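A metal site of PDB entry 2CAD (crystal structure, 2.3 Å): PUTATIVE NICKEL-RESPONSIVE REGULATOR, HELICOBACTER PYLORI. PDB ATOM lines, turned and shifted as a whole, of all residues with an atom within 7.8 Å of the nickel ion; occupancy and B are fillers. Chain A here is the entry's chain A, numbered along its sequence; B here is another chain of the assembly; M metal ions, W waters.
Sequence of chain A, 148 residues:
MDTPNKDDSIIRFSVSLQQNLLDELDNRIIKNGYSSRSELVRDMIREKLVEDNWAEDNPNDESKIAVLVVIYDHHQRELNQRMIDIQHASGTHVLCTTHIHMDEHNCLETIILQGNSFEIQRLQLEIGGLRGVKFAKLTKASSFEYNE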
ATOM      1  N   HIS A  74      19.800 -17.644  29.031  1.00  0.00           N
ATOM      2  CA  HIS A  74      19.446 -16.384  28.432  1.00  0.00           C
ATOM      3  C   HIS A  74      18.736 -16.500  27.031  1.00  0.00           C
ATOM      4  O   HIS A  74      17.832 -15.722  26.690  1.00  0.00           O
ATOM      5  CB  HIS A  74      20.760 -15.566  28.341  1.00  0.00           C
ATOM      6  CG  HIS A  74      20.569 -14.163  27.850  1.00  0.00           C
ATOM      7  ND1 HIS A  74      21.157 -13.707  26.690  1.00  0.00           N
ATOM      8  CD2 HIS A  74      19.845 -13.139  28.347  1.00  0.00           C
ATOM      9  CE1 HIS A  74      20.801 -12.444  26.491  1.00  0.00           C
ATOM     10  NE2 HIS A  74      20.006 -12.074  27.493  1.00  0.00           N
ATOM     11  N   HIS A  75      19.147 -17.490  26.238  1.00  0.00           N
ATOM     12  CA  HIS A  75      18.652 -17.615  24.860  1.00  0.00           C
ATOM     13  C   HIS A  75      17.333 -18.364  24.758  1.00  0.00           C
ATOM     14  O   HIS A  75      16.740 -18.410  23.689  1.00  0.00           O
ATOM     15  CB  HIS A  75      19.690 -18.308  23.971  1.00  0.00           C
ATOM     16  CG  HIS A  75      20.983 -17.563  23.878  1.00  0.00           C
ATOM     17  ND1 HIS A  75      22.210 -18.198  23.878  1.00  0.00           N
ATOM     18  CD2 HIS A  75      21.238 -16.233  23.818  1.00  0.00           C
ATOM     19  CE1 HIS A  75      23.168 -17.284  23.792  1.00  0.00           C
ATOM     20  NE2 HIS A  75      22.608 -16.082  23.770  1.00  0.00           N
ATOM     21  N   HIS A 101      22.332 -10.338  34.366  1.00  0.00           N
ATOM     22  CA  HIS A 101      23.059 -11.174  33.435  1.00  0.00           C
ATOM     23  C   HIS A 101      24.375 -11.562  34.104  1.00  0.00           C
ATOM     24  O   HIS A 101      25.080 -10.702  34.577  1.00  0.00           O
ATOM     25  CB  HIS A 101      23.395 -10.408  32.145  1.00  0.00           C
ATOM     26  CG  HIS A 101      22.218 -10.128  31.287  1.00  0.00           C
ATOM     27  ND1 HIS A 101      21.153  -9.344  31.701  1.00  0.00           N
ATOM     28  CD2 HIS A 101      21.923 -10.519  30.019  1.00  0.00           C
ATOM     29  CE1 HIS A 101      20.251  -9.274  30.735  1.00  0.00           C
ATOM     30  NE2 HIS A 101      20.695  -9.962  29.700  1.00  0.00           N
ATOM     31  N   ASP A 103      26.594 -13.733  32.246  1.00  0.00           N
ATOM     32  CA  ASP A 103      27.362 -13.707  30.992  1.00  0.00           C
ATOM     33  C   ASP A 103      26.330 -13.639  29.870  1.00  0.00           C
ATOM     34  O   ASP A 103      25.177 -13.344  30.147  1.00  0.00           O
ATOM     35  CB  ASP A 103      28.307 -14.949  30.891  1.00  0.00           C
ATOM     36  CG  ASP A 103      27.622 -16.253  31.267  1.00  0.00           C
ATOM     37  OD1 ASP A 103      26.641 -16.578  30.571  1.00  0.00           O
ATOM     38  OD2 ASP A 103      28.036 -16.965  32.214  1.00  0.00           O
ATOM     39  N   GLU A 104      26.693 -13.914  28.613  1.00  0.00           N
ATOM     40  CA  GLU A 104      25.722 -13.820  27.498  1.00  0.00           C
ATOM     41  C   GLU A 104      24.878 -15.075  27.390  1.00  0.00           C
ATOM     42  O   GLU A 104      23.854 -15.094  26.673  1.00  0.00           O
ATOM     43  CB  GLU A 104      26.424 -13.543  26.161  1.00  0.00           C
ATOM     44  N   CYS A 107      21.619 -15.950  32.963  1.00  0.00           N
ATOM     45  CA  CYS A 107      21.123 -14.962  33.866  1.00  0.00           C
ATOM     46  C   CYS A 107      20.956 -15.587  35.237  1.00  0.00           C
ATOM     47  O   CYS A 107      20.758 -16.798  35.343  1.00  0.00           O
ATOM     48  CB  CYS A 107      19.762 -14.448  33.386  1.00  0.00           C
ATOM     49  SG  CYS A 107      19.794 -13.575  31.822  1.00  0.00           S
ATOM     50  N   ILE B  84      11.631  -8.274  25.855  1.00  0.00           N
ATOM     51  CA  ILE B  84      13.017  -8.797  25.781  1.00  0.00           C
ATOM     52  C   ILE B  84      13.622  -8.675  24.367  1.00  0.00           C
ATOM     53  O   ILE B  84      14.798  -8.237  24.204  1.00  0.00           O
ATOM     54  CB  ILE B  84      13.076 -10.261  26.300  1.00  0.00           C
ATOM     55  CG1 ILE B  84      12.919 -10.252  27.827  1.00  0.00           C
ATOM     56  CG2 ILE B  84      14.399 -10.946  25.954  1.00  0.00           C
ATOM     57  CD1 ILE B  84      12.470 -11.542  28.399  1.00  0.00           C
ATOM     58  N   GLN B  87      14.269  -5.034  23.558  1.00  0.00           N
ATOM     59  CA  GLN B  87      15.427  -4.567  24.307  1.00  0.00           C
ATOM     60  C   GLN B  87      16.724  -5.097  23.724  1.00  0.00           C
ATOM     61  O   GLN B  87      17.696  -4.356  23.567  1.00  0.00           O
ATOM     62  CB  GLN B  87      15.265  -4.944  25.787  1.00  0.00           C
ATOM     63  CG  GLN B  87      16.402  -4.493  26.656  1.00  0.00           C
ATOM     64  CD  GLN B  87      17.587  -5.420  26.538  1.00  0.00           C
ATOM     65  OE1 GLN B  87      17.445  -6.635  26.658  1.00  0.00           O
ATOM     66  NE2 GLN B  87      18.762  -4.856  26.291  1.00  0.00           N
ATOM     67  N   HIS B  88      16.753  -6.371  23.371  1.00  0.00           N
ATOM     68  CA  HIS B  88      17.928  -6.928  22.700  1.00  0.00           C
ATOM     69  C   HIS B  88      18.239  -6.216  21.384  1.00  0.00           C
ATOM     70  O   HIS B  88      19.404  -5.905  21.113  1.00  0.00           O
ATOM     71  CB  HIS B  88      17.744  -8.411  22.417  1.00  0.00           C
ATOM     72  CG  HIS B  88      17.906  -9.273  23.628  1.00  0.00           C
ATOM     73  ND1 HIS B  88      17.114 -10.374  23.869  1.00  0.00           N
ATOM     74  CD2 HIS B  88      18.773  -9.201  24.668  1.00  0.00           C
ATOM     75  CE1 HIS B  88      17.476 -10.929  25.017  1.00  0.00           C
ATOM     76  NE2 HIS B  88      18.479 -10.240  25.517  1.00  0.00           N
ATOM     77  N   THR B  92      20.661  -1.466  23.837  1.00  0.00           N
ATOM     78  CA  THR B  92      20.848  -1.097  25.256  1.00  0.00           C
ATOM     79  C   THR B  92      21.290  -2.316  26.079  1.00  0.00           C
ATOM     80  O   THR B  92      20.964  -3.454  25.737  1.00  0.00           O
ATOM     81  CB  THR B  92      19.568  -0.563  25.887  1.00  0.00           C
ATOM     82  OG1 THR B  92      18.586  -1.603  25.919  1.00  0.00           O
ATOM     83  CG2 THR B  92      19.002   0.576  25.101  1.00  0.00           C
ATOM     84  N   HIS B  93      22.049  -2.072  27.154  1.00  0.00           N
ATOM     85  CA  HIS B  93      22.385  -3.132  28.129  1.00  0.00           C
ATOM     86  C   HIS B  93      21.480  -3.022  29.346  1.00  0.00           C
ATOM     87  O   HIS B  93      21.344  -1.958  29.905  1.00  0.00           O
ATOM     88  CB  HIS B  93      23.857  -3.056  28.545  1.00  0.00           C
ATOM     89  CG  HIS B  93      24.809  -3.207  27.399  1.00  0.00           C
ATOM     90  ND1 HIS B  93      24.812  -4.328  26.597  1.00  0.00           N
ATOM     91  CD2 HIS B  93      25.721  -2.363  26.867  1.00  0.00           C
ATOM     92  CE1 HIS B  93      25.716  -4.183  25.634  1.00  0.00           C
ATOM     93  NE2 HIS B  93      26.286  -2.991  25.787  1.00  0.00           N
ATOM     94  N   VAL B  94      20.842  -4.121  29.705  1.00  0.00           N
ATOM     95  CA  VAL B  94      20.074  -4.207  30.955  1.00  0.00           C
ATOM     96  C   VAL B  94      21.039  -4.625  32.063  1.00  0.00           C
ATOM     97  O   VAL B  94      21.604  -5.710  32.010  1.00  0.00           O
ATOM     98  CB  VAL B  94      18.938  -5.220  30.854  1.00  0.00           C
ATOM     99  CG1 VAL B  94      18.165  -5.272  32.174  1.00  0.00           C
ATOM    100  CG2 VAL B  94      18.010  -4.841  29.704  1.00  0.00           C
HETATM  101 NI    NI M   1      19.500 -10.053  27.626  1.00  0.00          NI
HETATM  102  O   HOH W   1      18.734  -8.036  28.329  1.00  0.00           O
HETATM  103  O   HOH W   2      21.308  -9.600  26.809  1.00  0.00           O
HETATM  104  O   HOH W   3      17.693 -10.758  28.437  1.00  0.00           O
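Three residues have an atom within 4 Å of the nickel ion: His 74, His 101 and His 88 of chain B. The nearest printed residue that does not touch the nickel ion is Gln 87 of chain B (4.1 Å).
The backbone carbonyl oxygen of Ile 84 of chain B is in hydrogen-bond range of a ring nitrogen (ND1) of His 88 of chain B. ND1 of His 74 sits at hydrogen-bond distance from O of Glu 104, 3.0 Å away.
The nickel ion is bound by water W2, 2.0 Å away. The nickel ion is bound by a ring nitrogen (NE2) of His 74, 2.1 Å away. The nickel ion is bound by water W3, 2.1 Å away. Water W1 binds the nickel ion (2.3 Å). NE2 of His 88 of chain B binds the nickel ion, at 2.4 Å. NE2 of His 101 is bound to the nickel ion (2.4 Å). The nickel ion has six donor atoms within binding distance.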
